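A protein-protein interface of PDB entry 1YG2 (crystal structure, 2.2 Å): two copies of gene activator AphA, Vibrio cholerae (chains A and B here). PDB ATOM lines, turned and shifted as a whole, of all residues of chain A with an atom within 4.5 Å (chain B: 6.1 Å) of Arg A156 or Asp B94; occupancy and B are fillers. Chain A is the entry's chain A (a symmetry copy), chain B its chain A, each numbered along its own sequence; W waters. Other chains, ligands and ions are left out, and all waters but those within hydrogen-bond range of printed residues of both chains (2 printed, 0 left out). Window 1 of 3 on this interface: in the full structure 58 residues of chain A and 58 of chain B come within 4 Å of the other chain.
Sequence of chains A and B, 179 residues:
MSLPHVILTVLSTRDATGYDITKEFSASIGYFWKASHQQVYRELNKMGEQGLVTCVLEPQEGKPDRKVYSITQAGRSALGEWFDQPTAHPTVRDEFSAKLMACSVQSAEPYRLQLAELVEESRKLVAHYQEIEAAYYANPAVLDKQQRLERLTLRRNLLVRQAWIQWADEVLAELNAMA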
ATOM      1  N   PHE A  32     -17.104  24.862  30.583  1.00  0.00           N
ATOM      2  CA  PHE A  32     -17.270  24.178  29.308  1.00  0.00           C
ATOM      3  C   PHE A  32     -16.910  24.997  28.077  1.00  0.00           C
ATOM      4  O   PHE A  32     -16.841  24.467  26.971  1.00  0.00           O
ATOM      5  CB  PHE A  32     -18.719  23.697  29.193  1.00  0.00           C
ATOM      6  CG  PHE A  32     -19.714  24.816  29.073  1.00  0.00           C
ATOM      7  CD1 PHE A  32     -20.065  25.320  27.824  1.00  0.00           C
ATOM      8  CD2 PHE A  32     -20.274  25.388  30.204  1.00  0.00           C
ATOM      9  CE1 PHE A  32     -20.963  26.386  27.704  1.00  0.00           C
ATOM     10  CE2 PHE A  32     -21.168  26.453  30.100  1.00  0.00           C
ATOM     11  CZ  PHE A  32     -21.513  26.952  28.844  1.00  0.00           C
ATOM     12  N   TRP A  33     -16.696  26.292  28.250  1.00  0.00           N
ATOM     13  CA  TRP A  33     -16.332  27.099  27.102  1.00  0.00           C
ATOM     14  C   TRP A  33     -15.288  28.143  27.474  1.00  0.00           C
ATOM     15  O   TRP A  33     -15.540  29.053  28.257  1.00  0.00           O
ATOM     16  CB  TRP A  33     -17.572  27.765  26.499  1.00  0.00           C
ATOM     17  CG  TRP A  33     -17.356  28.176  25.093  1.00  0.00           C
ATOM     18  CD1 TRP A  33     -16.691  29.283  24.653  1.00  0.00           C
ATOM     19  CD2 TRP A  33     -17.717  27.437  23.930  1.00  0.00           C
ATOM     20  NE1 TRP A  33     -16.614  29.278  23.282  1.00  0.00           N
ATOM     21  CE2 TRP A  33     -17.239  28.148  22.810  1.00  0.00           C
ATOM     22  CE3 TRP A  33     -18.402  26.230  23.718  1.00  0.00           C
ATOM     23  CZ2 TRP A  33     -17.421  27.703  21.499  1.00  0.00           C
ATOM     24  CZ3 TRP A  33     -18.585  25.783  22.414  1.00  0.00           C
ATOM     25  CH2 TRP A  33     -18.094  26.519  21.322  1.00  0.00           C
ATOM     26  N   LEU A 152     -23.867  20.198  36.201  1.00  0.00           N
ATOM     27  CA  LEU A 152     -23.637  19.171  35.193  1.00  0.00           C
ATOM     28  C   LEU A 152     -22.485  19.526  34.243  1.00  0.00           C
ATOM     29  O   LEU A 152     -21.688  18.659  33.890  1.00  0.00           O
ATOM     30  CB  LEU A 152     -24.932  18.910  34.416  1.00  0.00           C
ATOM     31  CG  LEU A 152     -26.026  18.198  35.225  1.00  0.00           C
ATOM     32  CD1 LEU A 152     -27.346  18.244  34.470  1.00  0.00           C
ATOM     33  CD2 LEU A 152     -25.609  16.754  35.501  1.00  0.00           C
ATOM     34  N   THR A 153     -22.377  20.789  33.829  1.00  0.00           N
ATOM     35  CA  THR A 153     -21.282  21.155  32.939  1.00  0.00           C
ATOM     36  C   THR A 153     -19.966  20.989  33.687  1.00  0.00           C
ATOM     37  O   THR A 153     -18.966  20.572  33.106  1.00  0.00           O
ATOM     38  CB  THR A 153     -21.392  22.598  32.435  1.00  0.00           C
ATOM     39  OG1 THR A 153     -21.343  23.494  33.546  1.00  0.00           O
ATOM     40  CG2 THR A 153     -22.686  22.788  31.652  1.00  0.00           C
ATOM     41  N   LEU A 154     -19.970  21.313  34.978  1.00  0.00           N
ATOM     42  CA  LEU A 154     -18.761  21.157  35.786  1.00  0.00           C
ATOM     43  C   LEU A 154     -18.412  19.666  35.839  1.00  0.00           C
ATOM     44  O   LEU A 154     -17.261  19.273  35.637  1.00  0.00           O
ATOM     45  CB  LEU A 154     -18.984  21.687  37.220  1.00  0.00           C
ATOM     46  CG  LEU A 154     -17.849  21.420  38.223  1.00  0.00           C
ATOM     47  CD1 LEU A 154     -16.568  22.027  37.710  1.00  0.00           C
ATOM     48  CD2 LEU A 154     -18.184  22.009  39.582  1.00  0.00           C
ATOM     49  N   ARG A 155     -19.420  18.837  36.089  1.00  0.00           N
ATOM     50  CA  ARG A 155     -19.217  17.394  36.186  1.00  0.00           C
ATOM     51  C   ARG A 155     -18.615  16.775  34.925  1.00  0.00           C
ATOM     52  O   ARG A 155     -17.925  15.757  35.001  1.00  0.00           O
ATOM     53  CB  ARG A 155     -20.544  16.690  36.494  1.00  0.00           C
ATOM     54  CG  ARG A 155     -21.276  17.202  37.727  1.00  0.00           C
ATOM     55  CD  ARG A 155     -20.985  16.367  38.934  1.00  0.00           C
ATOM     56  NE  ARG A 155     -21.136  14.947  38.635  1.00  0.00           N
ATOM     57  CZ  ARG A 155     -20.420  14.004  39.232  1.00  0.00           C
ATOM     58  NH1 ARG A 155     -19.528  14.354  40.155  1.00  0.00           N
ATOM     59  NH2 ARG A 155     -20.557  12.730  38.885  1.00  0.00           N
ATOM     60  N   ARG A 156     -18.868  17.371  33.763  1.00  0.00           N
ATOM     61  CA  ARG A 156     -18.329  16.804  32.526  1.00  0.00           C
ATOM     62  C   ARG A 156     -16.803  16.841  32.487  1.00  0.00           C
ATOM     63  O   ARG A 156     -16.165  15.849  32.140  1.00  0.00           O
ATOM     64  CB  ARG A 156     -18.885  17.533  31.301  1.00  0.00           C
ATOM     65  CG  ARG A 156     -18.715  16.731  30.019  1.00  0.00           C
ATOM     66  CD  ARG A 156     -18.540  17.611  28.797  1.00  0.00           C
ATOM     67  NE  ARG A 156     -17.242  17.359  28.182  1.00  0.00           N
ATOM     68  CZ  ARG A 156     -16.182  18.148  28.313  1.00  0.00           C
ATOM     69  NH1 ARG A 156     -16.266  19.259  29.032  1.00  0.00           N
ATOM     70  NH2 ARG A 156     -15.027  17.807  27.756  1.00  0.00           N
ATOM     71  N   ASN A 157     -16.216  17.985  32.832  1.00  0.00           N
ATOM     72  CA  ASN A 157     -14.757  18.118  32.821  1.00  0.00           C
ATOM     73  C   ASN A 157     -14.194  17.091  33.758  1.00  0.00           C
ATOM     74  O   ASN A 157     -13.222  16.406  33.459  1.00  0.00           O
ATOM     75  CB  ASN A 157     -14.303  19.473  33.360  1.00  0.00           C
ATOM     76  CG  ASN A 157     -14.879  20.624  32.605  1.00  0.00           C
ATOM     77  OD1 ASN A 157     -14.521  20.867  31.451  1.00  0.00           O
ATOM     78  ND2 ASN A 157     -15.786  21.353  33.249  1.00  0.00           N
ATOM     79  N   LEU A 158     -14.823  17.009  34.914  1.00  0.00           N
ATOM     80  CA  LEU A 158     -14.394  16.104  35.955  1.00  0.00           C
ATOM     81  C   LEU A 158     -14.300  14.656  35.496  1.00  0.00           C
ATOM     82  O   LEU A 158     -13.219  14.055  35.514  1.00  0.00           O
ATOM     83  CB  LEU A 158     -15.348  16.216  37.141  1.00  0.00           C
ATOM     84  CG  LEU A 158     -14.831  15.651  38.459  1.00  0.00           C
ATOM     85  CD1 LEU A 158     -13.578  16.411  38.869  1.00  0.00           C
ATOM     86  CD2 LEU A 158     -15.912  15.782  39.530  1.00  0.00           C
ATOM     87  N   LEU A 159     -15.427  14.102  35.071  1.00  0.00           N
ATOM     88  CA  LEU A 159     -15.485  12.713  34.636  1.00  0.00           C
ATOM     89  C   LEU A 159     -14.551  12.404  33.479  1.00  0.00           C
ATOM     90  O   LEU A 159     -13.826  11.406  33.504  1.00  0.00           O
ATOM     91  CB  LEU A 159     -16.926  12.354  34.273  1.00  0.00           C
ATOM     92  CG  LEU A 159     -17.879  12.408  35.474  1.00  0.00           C
ATOM     93  CD1 LEU A 159     -19.326  12.203  35.038  1.00  0.00           C
ATOM     94  CD2 LEU A 159     -17.467  11.330  36.472  1.00  0.00           C
ATOM     95  N   VAL A 160     -14.559  13.261  32.467  1.00  0.00           N
ATOM     96  CA  VAL A 160     -13.707  13.051  31.311  1.00  0.00           C
ATOM     97  C   VAL A 160     -12.238  13.181  31.684  1.00  0.00           C
ATOM     98  O   VAL A 160     -11.435  12.284  31.411  1.00  0.00           O
ATOM     99  CB  VAL A 160     -14.037  14.055  30.193  1.00  0.00           C
ATOM    100  CG1 VAL A 160     -13.035  13.922  29.065  1.00  0.00           C
ATOM    101  CG2 VAL A 160     -15.436  13.797  29.672  1.00  0.00           C
ATOM    102  N   THR B  91      -8.406  23.003  23.588  1.00  0.00           N
ATOM    103  CA  THR B  91      -9.170  23.978  24.356  1.00  0.00           C
ATOM    104  C   THR B  91     -10.586  23.467  24.586  1.00  0.00           C
ATOM    105  O   THR B  91     -11.206  22.899  23.686  1.00  0.00           O
ATOM    106  CB  THR B  91      -9.229  25.338  23.625  1.00  0.00           C
ATOM    107  OG1 THR B  91      -7.896  25.796  23.363  1.00  0.00           O
ATOM    108  CG2 THR B  91      -9.957  26.380  24.476  1.00  0.00           C
ATOM    109  N   VAL B  92     -11.093  23.668  25.796  1.00  0.00           N
ATOM    110  CA  VAL B  92     -12.427  23.209  26.137  1.00  0.00           C
ATOM    111  C   VAL B  92     -13.526  24.122  25.607  1.00  0.00           C
ATOM    112  O   VAL B  92     -13.622  25.291  25.982  1.00  0.00           O
ATOM    113  CB  VAL B  92     -12.608  23.092  27.666  1.00  0.00           C
ATOM    114  CG1 VAL B  92     -13.957  22.464  27.975  1.00  0.00           C
ATOM    115  CG2 VAL B  92     -11.470  22.274  28.278  1.00  0.00           C
ATOM    116  N   ARG B  93     -14.347  23.571  24.725  1.00  0.00           N
ATOM    117  CA  ARG B  93     -15.475  24.280  24.141  1.00  0.00           C
ATOM    118  C   ARG B  93     -16.474  23.163  23.876  1.00  0.00           C
ATOM    119  O   ARG B  93     -16.672  22.749  22.733  1.00  0.00           O
ATOM    120  CB  ARG B  93     -15.083  24.959  22.821  1.00  0.00           C
ATOM    121  CG  ARG B  93     -14.071  26.112  22.934  1.00  0.00           C
ATOM    122  CD  ARG B  93     -13.709  26.627  21.539  1.00  0.00           C
ATOM    123  NE  ARG B  93     -12.466  27.396  21.503  1.00  0.00           N
ATOM    124  CZ  ARG B  93     -12.318  28.595  22.049  1.00  0.00           C
ATOM    125  NH1 ARG B  93     -13.341  29.160  22.674  1.00  0.00           N
ATOM    126  NH2 ARG B  93     -11.156  29.229  21.965  1.00  0.00           N
ATOM    127  N   ASP B  94     -17.100  22.670  24.939  1.00  0.00           N
ATOM    128  CA  ASP B  94     -18.039  21.569  24.811  1.00  0.00           C
ATOM    129  C   ASP B  94     -19.431  21.933  24.319  1.00  0.00           C
ATOM    130  O   ASP B  94     -20.214  22.587  25.014  1.00  0.00           O
ATOM    131  CB  ASP B  94     -18.149  20.821  26.135  1.00  0.00           C
ATOM    132  CG  ASP B  94     -18.971  19.565  26.009  1.00  0.00           C
ATOM    133  OD1 ASP B  94     -20.119  19.539  26.482  1.00  0.00           O
ATOM    134  OD2 ASP B  94     -18.466  18.594  25.419  1.00  0.00           O
ATOM    135  N   GLU B  95     -19.744  21.459  23.118  1.00  0.00           N
ATOM    136  CA  GLU B  95     -21.030  21.724  22.496  1.00  0.00           C
ATOM    137  C   GLU B  95     -22.199  21.137  23.278  1.00  0.00           C
ATOM    138  O   GLU B  95     -23.267  21.739  23.356  1.00  0.00           O
ATOM    139  CB  GLU B  95     -21.042  21.175  21.069  1.00  0.00           C
ATOM    140  CG  GLU B  95     -22.166  21.738  20.221  1.00  0.00           C
ATOM    141  CD  GLU B  95     -21.925  23.183  19.815  1.00  0.00           C
ATOM    142  OE1 GLU B  95     -21.029  23.834  20.395  1.00  0.00           O
ATOM    143  OE2 GLU B  95     -22.641  23.667  18.914  1.00  0.00           O
ATOM    144  N   PHE B  96     -22.011  19.960  23.856  1.00  0.00           N
ATOM    145  CA  PHE B  96     -23.089  19.341  24.619  1.00  0.00           C
ATOM    146  C   PHE B  96     -23.411  20.155  25.855  1.00  0.00           C
ATOM    147  O   PHE B  96     -24.575  20.316  26.223  1.00  0.00           O
ATOM    148  CB  PHE B  96     -22.703  17.923  25.031  1.00  0.00           C
ATOM    149  CG  PHE B  96     -22.568  16.988  23.875  1.00  0.00           C
ATOM    150  CD1 PHE B  96     -21.315  16.539  23.467  1.00  0.00           C
ATOM    151  CD2 PHE B  96     -23.696  16.571  23.181  1.00  0.00           C
ATOM    152  CE1 PHE B  96     -21.186  15.691  22.378  1.00  0.00           C
ATOM    153  CE2 PHE B  96     -23.585  15.723  22.088  1.00  0.00           C
ATOM    154  CZ  PHE B  96     -22.326  15.279  21.685  1.00  0.00           C
ATOM    155  N   SER B  97     -22.369  20.667  26.499  1.00  0.00           N
ATOM    156  CA  SER B  97     -22.548  21.477  27.696  1.00  0.00           C
ATOM    157  C   SER B  97     -23.208  22.786  27.298  1.00  0.00           C
ATOM    158  O   SER B  97     -24.115  23.264  27.977  1.00  0.00           O
ATOM    159  CB  SER B  97     -21.204  21.759  28.363  1.00  0.00           C
ATOM    160  OG  SER B  97     -20.634  20.558  28.863  1.00  0.00           O
ATOM    161  N   ALA B  98     -22.748  23.355  26.189  1.00  0.00           N
ATOM    162  CA  ALA B  98     -23.305  24.601  25.690  1.00  0.00           C
ATOM    163  C   ALA B  98     -24.810  24.452  25.424  1.00  0.00           C
ATOM    164  O   ALA B  98     -25.587  25.326  25.768  1.00  0.00           O
ATOM    165  CB  ALA B  98     -22.580  25.014  24.416  1.00  0.00           C
ATOM    166  N   LYS B  99     -25.216  23.339  24.821  1.00  0.00           N
ATOM    167  CA  LYS B  99     -26.631  23.109  24.548  1.00  0.00           C
ATOM    168  C   LYS B  99     -27.379  22.898  25.867  1.00  0.00           C
ATOM    169  O   LYS B  99     -28.494  23.381  26.044  1.00  0.00           O
ATOM    170  CB  LYS B  99     -26.817  21.870  23.665  1.00  0.00           C
ATOM    171  CG  LYS B  99     -26.282  21.986  22.239  1.00  0.00           C
ATOM    172  CD  LYS B  99     -27.146  22.862  21.363  1.00  0.00           C
ATOM    173  CE  LYS B  99     -26.642  22.883  19.906  1.00  0.00           C
ATOM    174  NZ  LYS B  99     -26.922  21.619  19.159  1.00  0.00           N
ATOM    175  N   TRP B 164     -17.952   9.663  29.213  1.00  0.00           N
ATOM    176  CA  TRP B 164     -18.959  10.524  28.608  1.00  0.00           C
ATOM    177  C   TRP B 164     -20.374   9.947  28.769  1.00  0.00           C
ATOM    178  O   TRP B 164     -21.341  10.688  28.977  1.00  0.00           O
ATOM    179  CB  TRP B 164     -18.649  10.743  27.130  1.00  0.00           C
ATOM    180  CG  TRP B 164     -19.562  11.736  26.509  1.00  0.00           C
ATOM    181  CD1 TRP B 164     -19.395  13.095  26.456  1.00  0.00           C
ATOM    182  CD2 TRP B 164     -20.823  11.460  25.889  1.00  0.00           C
ATOM    183  NE1 TRP B 164     -20.477  13.678  25.837  1.00  0.00           N
ATOM    184  CE2 TRP B 164     -21.366  12.702  25.480  1.00  0.00           C
ATOM    185  CE3 TRP B 164     -21.546  10.285  25.639  1.00  0.00           C
ATOM    186  CZ2 TRP B 164     -22.602  12.800  24.833  1.00  0.00           C
ATOM    187  CZ3 TRP B 164     -22.778  10.385  24.993  1.00  0.00           C
ATOM    188  CH2 TRP B 164     -23.292  11.636  24.597  1.00  0.00           C
ATOM    189  N   TRP B 167     -21.590  10.596  32.166  1.00  0.00           N
ATOM    190  CA  TRP B 167     -22.035  11.983  32.256  1.00  0.00           C
ATOM    191  C   TRP B 167     -23.400  12.186  31.597  1.00  0.00           C
ATOM    192  O   TRP B 167     -24.296  12.806  32.166  1.00  0.00           O
ATOM    193  CB  TRP B 167     -21.027  12.914  31.578  1.00  0.00           C
ATOM    194  CG  TRP B 167     -21.472  14.331  31.610  1.00  0.00           C
ATOM    195  CD1 TRP B 167     -21.591  15.122  32.714  1.00  0.00           C
ATOM    196  CD2 TRP B 167     -21.929  15.111  30.504  1.00  0.00           C
ATOM    197  NE1 TRP B 167     -22.101  16.349  32.365  1.00  0.00           N
ATOM    198  CE2 TRP B 167     -22.321  16.369  31.011  1.00  0.00           C
ATOM    199  CE3 TRP B 167     -22.058  14.869  29.127  1.00  0.00           C
ATOM    200  CZ2 TRP B 167     -22.825  17.389  30.199  1.00  0.00           C
ATOM    201  CZ3 TRP B 167     -22.559  15.880  28.313  1.00  0.00           C
ATOM    202  CH2 TRP B 167     -22.941  17.127  28.857  1.00  0.00           C
HETATM  203  O   HOH W   1     -18.396  20.726  30.464  1.00  0.00           O
HETATM  204  O   HOH W   2     -18.665  15.998  25.558  1.00  0.00           O
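Phe A32 touches Ser B97.
CE1 of Phe A32 touches CA of Ala B98, at 3.6 Å.
O of Val B92 touches CA of Trp A33, at 3.4 Å.
CE3 of Trp A33 touches N of Asp B94 (3.98 Å).
CZ3 of Trp A33 touches OE1 of Glu B95 (3.7 Å).
Thr A153 touches Ser B97.
OG of Ser B97 touches CD of Arg A156, 3.6 Å away.
Arg A156 touches Trp B167 (CB to NE1, 3.6 Å).
OD1 of Asn A157 touches CG1 of Val B92 (3.9 Å).
CA of Trp B167 touches CD1 of Leu A159 (3.9 Å).
Water W2 lies within hydrogen-bond range of OD2 of Asp B94 (2.6 Å), NE1 of Trp B164 (3.0 Å) and NE of Arg A156 (3.3 Å).
Water W1 lies within hydrogen-bond range of the backbone carbonyl oxygen (O) of Thr A153 (2.7 Å), the side-chain hydroxyl (OG) of Ser B97 (2.8 Å) and the guanidinium group (NH1) of Arg A156 (3.0 Å).
Of the printed residues of chain B, Arg A156 touches Asp B94, Ser B97 and Trp B167.
Printed residues of chain B within 4 Å of Leu A159: Trp B167 (3.9 Å).
Printed residues of chain A within 4 Å of Arg B93: Phe A32 and Trp A33.
Printed residues of chain A within 4 Å of Asp B94: Phe A32, Trp A33 and Arg A156.
Of the printed residues of chain A, Glu B95 touches Trp A33.
Of the printed residues of chain A, Ala B98 touches Phe A32.
The nearest printed residue of chain B that does not touch Trp A33 is Ala B98 (4.4 Å).
Of the 11 printed residues of chain A, 7 touch a printed residue of chain B.
Hydrophobic or aromatic side chains of chain A that line the printed part of chain B: Phe A32, Trp A33 and Leu A159.
Of the 11 printed residues of chain B, 7 touch a printed residue of chain A.
Among the printed residues, 16 pairs touch across the chains.
Among the printed residues, Asp or Glu carboxylates within 4 Å of a Lys or Arg side-chain nitrogen of the other chain: Arg A156 with Asp B94 (3.3 Å).
The side-chain carboxylate of Asp B94 lies within hydrogen-bond range of the backbone NH of Phe B96.
The backbone NH (N) of Ser B97 is in hydrogen-bond range of the side-chain carboxylate (OD1) of Asp B94 (2.5 Å).
ND2 of Asn A157 sits at hydrogen-bond distance from O of Thr A153.
The backbone carbonyl oxygen (O) of Leu A154 sits at hydrogen-bond distance from the side-chain amide nitrogen (ND2) of Asn A157.
NH1 of Arg A156 sits at hydrogen-bond distance from OD1 of Asn A157 (3.4 Å).
O of Phe A32 sits close to N of Arg B93 (3.5 Å).
The backbone NH of Asp B94 sits at hydrogen-bond distance from the backbone carbonyl oxygen of Phe A32.
The side-chain carboxylate (OD2) of Asp B94 lies within salt-bridge range of the guanidinium group (NE) of Arg A156.
NE1 of Trp B167 lies within hydrogen-bond range of O of Leu A152 (2.8 Å).
O of Phe A32 lies close to O of Val B92, 3.5 Å away.
The indole nitrogen (NE1) of Trp A33 lies close to the guanidinium group (NH1) of Arg B93.
No position is printed for both chains.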
